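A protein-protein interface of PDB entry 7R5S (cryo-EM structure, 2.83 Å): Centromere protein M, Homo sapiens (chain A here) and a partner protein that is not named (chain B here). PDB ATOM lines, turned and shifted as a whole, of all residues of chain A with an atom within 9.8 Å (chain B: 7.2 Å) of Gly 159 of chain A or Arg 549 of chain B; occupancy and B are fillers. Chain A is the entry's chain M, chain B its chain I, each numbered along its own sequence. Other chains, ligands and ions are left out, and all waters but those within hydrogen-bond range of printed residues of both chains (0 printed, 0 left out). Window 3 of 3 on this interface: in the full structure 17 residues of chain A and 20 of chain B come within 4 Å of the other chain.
The side-chain carboxylate (OE2) of Glu 551 of chain B is in salt-bridge range of the guanidinium group (NH2) of Arg 148 of chain A, at 3.6 Å.
Among the printed residues, merely in contact across the chains: Leu 168 of chain A with Thr 546 of chain B (3.7 Å), Leu 168 of chain A with Trp 542 of chain B (3.8 Å), Val 160 of chain A with Leu 550 of chain B (3.8 Å), Ile 152 of chain A with Leu 550 of chain B (3.97 Å) and Gly 159 of chain A with Arg 549 of chain B (3.997 Å).
Of the printed residues of chain B, Gly 159 of chain A touches Arg 549.
Printed residues of chain B within 4 Å of Val 160 of chain A: Leu 550 (3.8 Å).
Of the printed residues of chain B, Leu 168 of chain A touches Trp 542 (3.8 Å) and Thr 546 (3.7 Å).
Of the printed residues of chain A, Trp 542 of chain B touches Leu 168.
Thr 546 of chain B touches just one residue of chain A: Leu 168 (3.7 Å).
No residue of chain A comes within 4 Å of Ala 547 of chain B.
Printed residues of chain A within 4 Å of Arg 549 of chain B: Gly 159 (3.997 Å).
The nearest printed residue of chain A that does not touch Trp 542 of chain B is Asn 164 of chain A (6.8 Å).
Along chain B the printed residues that touch a printed residue of chain A span positions 542 to 551.
Of the 15 printed residues of chain A, 5 touch a printed residue of chain B.
Among the printed residues, 6 pairs touch across the chains.
Among the printed residues, Asp or Glu carboxylates within 4 Å of a Lys or Arg side-chain nitrogen of the other chain: Arg 148 of chain A with Glu 551 of chain B (3.6 Å).
O of Trp 542 of chain B is in hydrogen-bond range of OG1 of Thr 546 of chain B, at 2.9 Å.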
ATOM      1  N   ARG A 148     -10.646  20.703 -10.916  1.00  0.00           N
ATOM      2  CA  ARG A 148     -12.046  21.120 -10.977  1.00  0.00           C
ATOM      3  C   ARG A 148     -12.959  20.101 -10.302  1.00  0.00           C
ATOM      4  O   ARG A 148     -13.879  20.471  -9.560  1.00  0.00           O
ATOM      5  CB  ARG A 148     -12.470  21.344 -12.428  1.00  0.00           C
ATOM      6  CG  ARG A 148     -11.711  22.459 -13.126  1.00  0.00           C
ATOM      7  CD  ARG A 148     -12.383  22.853 -14.429  1.00  0.00           C
ATOM      8  NE  ARG A 148     -13.635  23.570 -14.204  1.00  0.00           N
ATOM      9  CZ  ARG A 148     -13.728  24.891 -14.098  1.00  0.00           C
ATOM     10  NH1 ARG A 148     -12.641  25.644 -14.196  1.00  0.00           N
ATOM     11  NH2 ARG A 148     -14.908  25.460 -13.893  1.00  0.00           N
ATOM     12  N   GLN A 151     -12.595  20.491  -6.578  1.00  0.00           N
ATOM     13  CA  GLN A 151     -13.307  21.665  -6.085  1.00  0.00           C
ATOM     14  C   GLN A 151     -14.808  21.413  -6.032  1.00  0.00           C
ATOM     15  O   GLN A 151     -15.495  21.895  -5.124  1.00  0.00           O
ATOM     16  CB  GLN A 151     -12.999  22.878  -6.961  1.00  0.00           C
ATOM     17  CG  GLN A 151     -11.678  23.555  -6.645  1.00  0.00           C
ATOM     18  CD  GLN A 151     -11.500  24.858  -7.396  1.00  0.00           C
ATOM     19  OE1 GLN A 151     -12.145  25.090  -8.418  1.00  0.00           O
ATOM     20  NE2 GLN A 151     -10.624  25.717  -6.890  1.00  0.00           N
ATOM     21  N   ILE A 152     -15.337  20.662  -7.000  1.00  0.00           N
ATOM     22  CA  ILE A 152     -16.758  20.327  -6.978  1.00  0.00           C
ATOM     23  C   ILE A 152     -17.073  19.410  -5.800  1.00  0.00           C
ATOM     24  O   ILE A 152     -18.061  19.609  -5.084  1.00  0.00           O
ATOM     25  CB  ILE A 152     -17.185  19.694  -8.315  1.00  0.00           C
ATOM     26  CG1 ILE A 152     -17.214  20.750  -9.421  1.00  0.00           C
ATOM     27  CG2 ILE A 152     -18.544  19.026  -8.182  1.00  0.00           C
ATOM     28  CD1 ILE A 152     -17.710  20.226 -10.750  1.00  0.00           C
ATOM     29  N   GLY A 155     -17.222  20.810  -1.962  1.00  0.00           N
ATOM     30  CA  GLY A 155     -18.309  21.655  -1.513  1.00  0.00           C
ATOM     31  C   GLY A 155     -18.098  23.136  -1.716  1.00  0.00           C
ATOM     32  O   GLY A 155     -18.723  23.936  -1.010  1.00  0.00           O
ATOM     33  N   HIS A 156     -17.241  23.531  -2.655  1.00  0.00           N
ATOM     34  CA  HIS A 156     -16.968  24.934  -2.928  1.00  0.00           C
ATOM     35  C   HIS A 156     -17.796  25.479  -4.086  1.00  0.00           C
ATOM     36  O   HIS A 156     -17.577  26.619  -4.508  1.00  0.00           O
ATOM     37  CB  HIS A 156     -15.478  25.137  -3.211  1.00  0.00           C
ATOM     38  CG  HIS A 156     -14.596  24.867  -2.030  1.00  0.00           C
ATOM     39  ND1 HIS A 156     -15.092  24.486  -0.802  1.00  0.00           N
ATOM     40  CD2 HIS A 156     -13.251  24.927  -1.891  1.00  0.00           C
ATOM     41  CE1 HIS A 156     -14.090  24.322   0.043  1.00  0.00           C
ATOM     42  NE2 HIS A 156     -12.962  24.582  -0.593  1.00  0.00           N
ATOM     43  N   VAL A 157     -18.733  24.694  -4.607  1.00  0.00           N
ATOM     44  CA  VAL A 157     -19.615  25.140  -5.682  1.00  0.00           C
ATOM     45  C   VAL A 157     -21.052  25.085  -5.178  1.00  0.00           C
ATOM     46  O   VAL A 157     -21.589  23.989  -4.963  1.00  0.00           O
ATOM     47  CB  VAL A 157     -19.435  24.288  -6.948  1.00  0.00           C
ATOM     48  CG1 VAL A 157     -20.385  24.753  -8.039  1.00  0.00           C
ATOM     49  CG2 VAL A 157     -17.994  24.352  -7.428  1.00  0.00           C
ATOM     50  N   PRO A 158     -21.708  26.227  -4.972  1.00  0.00           N
ATOM     51  CA  PRO A 158     -23.077  26.209  -4.437  1.00  0.00           C
ATOM     52  C   PRO A 158     -24.052  25.597  -5.432  1.00  0.00           C
ATOM     53  O   PRO A 158     -24.137  26.026  -6.585  1.00  0.00           O
ATOM     54  CB  PRO A 158     -23.383  27.691  -4.187  1.00  0.00           C
ATOM     55  CG  PRO A 158     -22.045  28.369  -4.164  1.00  0.00           C
ATOM     56  CD  PRO A 158     -21.190  27.596  -5.115  1.00  0.00           C
ATOM     57  N   GLY A 159     -24.794  24.591  -4.974  1.00  0.00           N
ATOM     58  CA  GLY A 159     -25.805  23.940  -5.778  1.00  0.00           C
ATOM     59  C   GLY A 159     -25.390  22.617  -6.385  1.00  0.00           C
ATOM     60  O   GLY A 159     -26.259  21.879  -6.865  1.00  0.00           O
ATOM     61  N   VAL A 160     -24.099  22.293  -6.379  1.00  0.00           N
ATOM     62  CA  VAL A 160     -23.587  21.055  -6.957  1.00  0.00           C
ATOM     63  C   VAL A 160     -22.800  20.315  -5.885  1.00  0.00           C
ATOM     64  O   VAL A 160     -21.916  20.894  -5.246  1.00  0.00           O
ATOM     65  CB  VAL A 160     -22.709  21.323  -8.193  1.00  0.00           C
ATOM     66  CG1 VAL A 160     -22.216  20.014  -8.787  1.00  0.00           C
ATOM     67  CG2 VAL A 160     -23.477  22.128  -9.229  1.00  0.00           C
ATOM     68  N   SER A 161     -23.122  19.041  -5.694  1.00  0.00           N
ATOM     69  CA  SER A 161     -22.455  18.179  -4.729  1.00  0.00           C
ATOM     70  C   SER A 161     -21.907  16.945  -5.440  1.00  0.00           C
ATOM     71  O   SER A 161     -22.018  16.801  -6.659  1.00  0.00           O
ATOM     72  CB  SER A 161     -23.411  17.784  -3.600  1.00  0.00           C
ATOM     73  OG  SER A 161     -24.345  16.814  -4.039  1.00  0.00           O
ATOM     74  N   ALA A 162     -21.305  16.047  -4.657  1.00  0.00           N
ATOM     75  CA  ALA A 162     -20.759  14.820  -5.228  1.00  0.00           C
ATOM     76  C   ALA A 162     -21.868  13.898  -5.720  1.00  0.00           C
ATOM     77  O   ALA A 162     -21.705  13.204  -6.730  1.00  0.00           O
ATOM     78  CB  ALA A 162     -19.882  14.106  -4.201  1.00  0.00           C
ATOM     79  N   LEU A 163     -23.004  13.880  -5.019  1.00  0.00           N
ATOM     80  CA  LEU A 163     -24.126  13.055  -5.453  1.00  0.00           C
ATOM     81  C   LEU A 163     -24.689  13.535  -6.784  1.00  0.00           C
ATOM     82  O   LEU A 163     -25.198  12.729  -7.571  1.00  0.00           O
ATOM     83  CB  LEU A 163     -25.215  13.048  -4.381  1.00  0.00           C
ATOM     84  CG  LEU A 163     -26.270  11.946  -4.478  1.00  0.00           C
ATOM     85  CD1 LEU A 163     -25.612  10.575  -4.475  1.00  0.00           C
ATOM     86  CD2 LEU A 163     -27.269  12.064  -3.343  1.00  0.00           C
ATOM     87  N   ASN A 164     -24.610  14.840  -7.055  1.00  0.00           N
ATOM     88  CA  ASN A 164     -25.022  15.358  -8.354  1.00  0.00           C
ATOM     89  C   ASN A 164     -23.987  15.043  -9.427  1.00  0.00           C
ATOM     90  O   ASN A 164     -24.345  14.720 -10.565  1.00  0.00           O
ATOM     91  CB  ASN A 164     -25.259  16.866  -8.263  1.00  0.00           C
ATOM     92  CG  ASN A 164     -26.160  17.386  -9.367  1.00  0.00           C
ATOM     93  OD1 ASN A 164     -26.313  16.754 -10.410  1.00  0.00           O
ATOM     94  ND2 ASN A 164     -26.762  18.546  -9.137  1.00  0.00           N
ATOM     95  N   LEU A 165     -22.700  15.133  -9.080  1.00  0.00           N
ATOM     96  CA  LEU A 165     -21.649  14.753 -10.016  1.00  0.00           C
ATOM     97  C   LEU A 165     -21.748  13.282 -10.394  1.00  0.00           C
ATOM     98  O   LEU A 165     -21.353  12.896 -11.499  1.00  0.00           O
ATOM     99  CB  LEU A 165     -20.278  15.061  -9.416  1.00  0.00           C
ATOM    100  CG  LEU A 165     -19.060  14.879 -10.322  1.00  0.00           C
ATOM    101  CD1 LEU A 165     -19.136  15.819 -11.515  1.00  0.00           C
ATOM    102  CD2 LEU A 165     -17.777  15.100  -9.540  1.00  0.00           C
ATOM    103  N   LEU A 168     -24.141  13.409 -13.168  1.00  0.00           N
ATOM    104  CA  LEU A 168     -23.671  14.146 -14.337  1.00  0.00           C
ATOM    105  C   LEU A 168     -22.749  13.292 -15.200  1.00  0.00           C
ATOM    106  O   LEU A 168     -22.775  13.393 -16.432  1.00  0.00           O
ATOM    107  CB  LEU A 168     -22.961  15.427 -13.903  1.00  0.00           C
ATOM    108  CG  LEU A 168     -23.834  16.511 -13.271  1.00  0.00           C
ATOM    109  CD1 LEU A 168     -23.004  17.742 -12.943  1.00  0.00           C
ATOM    110  CD2 LEU A 168     -24.988  16.869 -14.191  1.00  0.00           C
ATOM    111  N   TRP B 542     -30.565  20.698 -21.223  1.00  0.00           N
ATOM    112  CA  TRP B 542     -30.075  20.209 -19.938  1.00  0.00           C
ATOM    113  C   TRP B 542     -28.600  20.547 -19.749  1.00  0.00           C
ATOM    114  O   TRP B 542     -28.182  20.970 -18.661  1.00  0.00           O
ATOM    115  CB  TRP B 542     -30.307  18.701 -19.836  1.00  0.00           C
ATOM    116  CG  TRP B 542     -29.601  18.040 -18.694  1.00  0.00           C
ATOM    117  CD1 TRP B 542     -29.891  18.165 -17.367  1.00  0.00           C
ATOM    118  CD2 TRP B 542     -28.492  17.137 -18.779  1.00  0.00           C
ATOM    119  NE1 TRP B 542     -29.028  17.400 -16.620  1.00  0.00           N
ATOM    120  CE2 TRP B 542     -28.159  16.759 -17.463  1.00  0.00           C
ATOM    121  CE3 TRP B 542     -27.746  16.614 -19.838  1.00  0.00           C
ATOM    122  CZ2 TRP B 542     -27.114  15.883 -17.180  1.00  0.00           C
ATOM    123  CZ3 TRP B 542     -26.709  15.744 -19.555  1.00  0.00           C
ATOM    124  CH2 TRP B 542     -26.403  15.388 -18.236  1.00  0.00           C
ATOM    125  N   LEU B 543     -27.799  20.360 -20.802  1.00  0.00           N
ATOM    126  CA  LEU B 543     -26.390  20.741 -20.748  1.00  0.00           C
ATOM    127  C   LEU B 543     -26.233  22.221 -20.420  1.00  0.00           C
ATOM    128  O   LEU B 543     -25.408  22.599 -19.582  1.00  0.00           O
ATOM    129  CB  LEU B 543     -25.704  20.418 -22.076  1.00  0.00           C
ATOM    130  CG  LEU B 543     -25.325  18.967 -22.369  1.00  0.00           C
ATOM    131  CD1 LEU B 543     -24.668  18.869 -23.733  1.00  0.00           C
ATOM    132  CD2 LEU B 543     -24.403  18.425 -21.292  1.00  0.00           C
ATOM    133  N   SER B 544     -27.020  23.074 -21.078  1.00  0.00           N
ATOM    134  CA  SER B 544     -26.915  24.513 -20.858  1.00  0.00           C
ATOM    135  C   SER B 544     -27.315  24.889 -19.437  1.00  0.00           C
ATOM    136  O   SER B 544     -26.671  25.738 -18.812  1.00  0.00           O
ATOM    137  CB  SER B 544     -27.777  25.262 -21.872  1.00  0.00           C
ATOM    138  OG  SER B 544     -27.605  24.733 -23.175  1.00  0.00           O
ATOM    139  N   THR B 545     -28.374  24.269 -18.911  1.00  0.00           N
ATOM    140  CA  THR B 545     -28.792  24.556 -17.542  1.00  0.00           C
ATOM    141  C   THR B 545     -27.710  24.161 -16.543  1.00  0.00           C
ATOM    142  O   THR B 545     -27.365  24.935 -15.637  1.00  0.00           O
ATOM    143  CB  THR B 545     -30.103  23.833 -17.229  1.00  0.00           C
ATOM    144  OG1 THR B 545     -31.126  24.288 -18.121  1.00  0.00           O
ATOM    145  CG2 THR B 545     -30.531  24.103 -15.796  1.00  0.00           C
ATOM    146  N   THR B 546     -27.151  22.957 -16.700  1.00  0.00           N
ATOM    147  CA  THR B 546     -26.108  22.518 -15.778  1.00  0.00           C
ATOM    148  C   THR B 546     -24.860  23.387 -15.898  1.00  0.00           C
ATOM    149  O   THR B 546     -24.206  23.687 -14.892  1.00  0.00           O
ATOM    150  CB  THR B 546     -25.767  21.050 -16.027  1.00  0.00           C
ATOM    151  OG1 THR B 546     -26.976  20.288 -16.124  1.00  0.00           O
ATOM    152  CG2 THR B 546     -24.929  20.504 -14.882  1.00  0.00           C
ATOM    153  N   ALA B 547     -24.524  23.820 -17.116  1.00  0.00           N
ATOM    154  CA  ALA B 547     -23.352  24.669 -17.297  1.00  0.00           C
ATOM    155  C   ALA B 547     -23.567  26.049 -16.687  1.00  0.00           C
ATOM    156  O   ALA B 547     -22.634  26.638 -16.132  1.00  0.00           O
ATOM    157  CB  ALA B 547     -23.014  24.786 -18.782  1.00  0.00           C
ATOM    158  N   MET B 548     -24.785  26.584 -16.789  1.00  0.00           N
ATOM    159  CA  MET B 548     -25.085  27.856 -16.144  1.00  0.00           C
ATOM    160  C   MET B 548     -25.012  27.730 -14.629  1.00  0.00           C
ATOM    161  O   MET B 548     -24.560  28.655 -13.943  1.00  0.00           O
ATOM    162  CB  MET B 548     -26.462  28.359 -16.576  1.00  0.00           C
ATOM    163  CG  MET B 548     -26.480  29.012 -17.945  1.00  0.00           C
ATOM    164  SD  MET B 548     -25.536  30.546 -18.000  1.00  0.00           S
ATOM    165  CE  MET B 548     -26.460  31.550 -16.842  1.00  0.00           C
ATOM    166  N   ARG B 549     -25.452  26.592 -14.086  1.00  0.00           N
ATOM    167  CA  ARG B 549     -25.323  26.381 -12.647  1.00  0.00           C
ATOM    168  C   ARG B 549     -23.864  26.236 -12.228  1.00  0.00           C
ATOM    169  O   ARG B 549     -23.487  26.681 -11.138  1.00  0.00           O
ATOM    170  CB  ARG B 549     -26.123  25.153 -12.215  1.00  0.00           C
ATOM    171  CG  ARG B 549     -26.160  24.944 -10.709  1.00  0.00           C
ATOM    172  CD  ARG B 549     -27.006  23.742 -10.321  1.00  0.00           C
ATOM    173  NE  ARG B 549     -28.421  23.942 -10.617  1.00  0.00           N
ATOM    174  CZ  ARG B 549     -29.067  23.347 -11.614  1.00  0.00           C
ATOM    175  NH1 ARG B 549     -28.425  22.507 -12.414  1.00  0.00           N
ATOM    176  NH2 ARG B 549     -30.356  23.589 -11.809  1.00  0.00           N
ATOM    177  N   LEU B 550     -23.031  25.629 -13.075  1.00  0.00           N
ATOM    178  CA  LEU B 550     -21.635  25.393 -12.715  1.00  0.00           C
ATOM    179  C   LEU B 550     -20.795  26.663 -12.820  1.00  0.00           C
ATOM    180  O   LEU B 550     -20.023  26.979 -11.909  1.00  0.00           O
ATOM    181  CB  LEU B 550     -21.044  24.293 -13.599  1.00  0.00           C
ATOM    182  CG  LEU B 550     -21.350  22.846 -13.213  1.00  0.00           C
ATOM    183  CD1 LEU B 550     -20.820  21.892 -14.268  1.00  0.00           C
ATOM    184  CD2 LEU B 550     -20.758  22.523 -11.853  1.00  0.00           C
ATOM    185  N   GLU B 551     -20.927  27.399 -13.923  1.00  0.00           N
ATOM    186  CA  GLU B 551     -20.070  28.547 -14.202  1.00  0.00           C
ATOM    187  C   GLU B 551     -20.493  29.814 -13.468  1.00  0.00           C
ATOM    188  O   GLU B 551     -19.978  30.891 -13.789  1.00  0.00           O
ATOM    189  CB  GLU B 551     -20.030  28.814 -15.709  1.00  0.00           C
ATOM    190  CG  GLU B 551     -19.255  27.775 -16.504  1.00  0.00           C
ATOM    191  CD  GLU B 551     -17.765  27.809 -16.216  1.00  0.00           C
ATOM    192  OE1 GLU B 551     -17.259  28.875 -15.810  1.00  0.00           O
ATOM    193  OE2 GLU B 551     -17.101  26.766 -16.395  1.00  0.00           O
ATOM    194  N   SER B 552     -21.414  29.712 -12.507  1.00  0.00           N
ATOM    195  CA  SER B 552     -21.816  30.841 -11.665  1.00  0.00           C
ATOM    196  C   SER B 552     -22.411  31.984 -12.486  1.00  0.00           C
ATOM    197  O   SER B 552     -22.100  33.156 -12.265  1.00  0.00           O
ATOM    198  CB  SER B 552     -20.646  31.338 -10.811  1.00  0.00           C
ATOM    199  OG  SER B 552     -20.388  30.453  -9.735  1.00  0.00           O
ATOM    200  N   ASN B 553     -23.272  31.635 -13.444  1.00  0.00           N
ATOM    201  CA  ASN B 553     -24.051  32.603 -14.219  1.00  0.00           C
ATOM    202  C   ASN B 553     -23.148  33.601 -14.948  1.00  0.00           C
ATOM    203  O   ASN B 553     -23.167  34.806 -14.692  1.00  0.00           O
ATOM    204  CB  ASN B 553     -25.061  33.329 -13.324  1.00  0.00           C
ATOM    205  CG  ASN B 553     -26.117  32.398 -12.764  1.00  0.00           C
ATOM    206  OD1 ASN B 553     -26.525  31.439 -13.418  1.00  0.00           O
ATOM    207  ND2 ASN B 553     -26.567  32.678 -11.547  1.00  0.00           N
ATOM    208  N   LEU B 557     -21.326  32.692 -21.582  1.00  0.00           N
ATOM    209  CA  LEU B 557     -21.968  31.440 -21.966  1.00  0.00           C
ATOM    210  C   LEU B 557     -23.440  31.625 -22.306  1.00  0.00           C
ATOM    211  O   LEU B 557     -23.959  30.942 -23.203  1.00  0.00           O
ATOM    212  CB  LEU B 557     -21.821  30.417 -20.838  1.00  0.00           C
ATOM    213  CG  LEU B 557     -22.261  28.980 -21.115  1.00  0.00           C
ATOM    214  CD1 LEU B 557     -21.333  28.320 -22.121  1.00  0.00           C
ATOM    215  CD2 LEU B 557     -22.300  28.192 -19.820  1.00  0.00           C
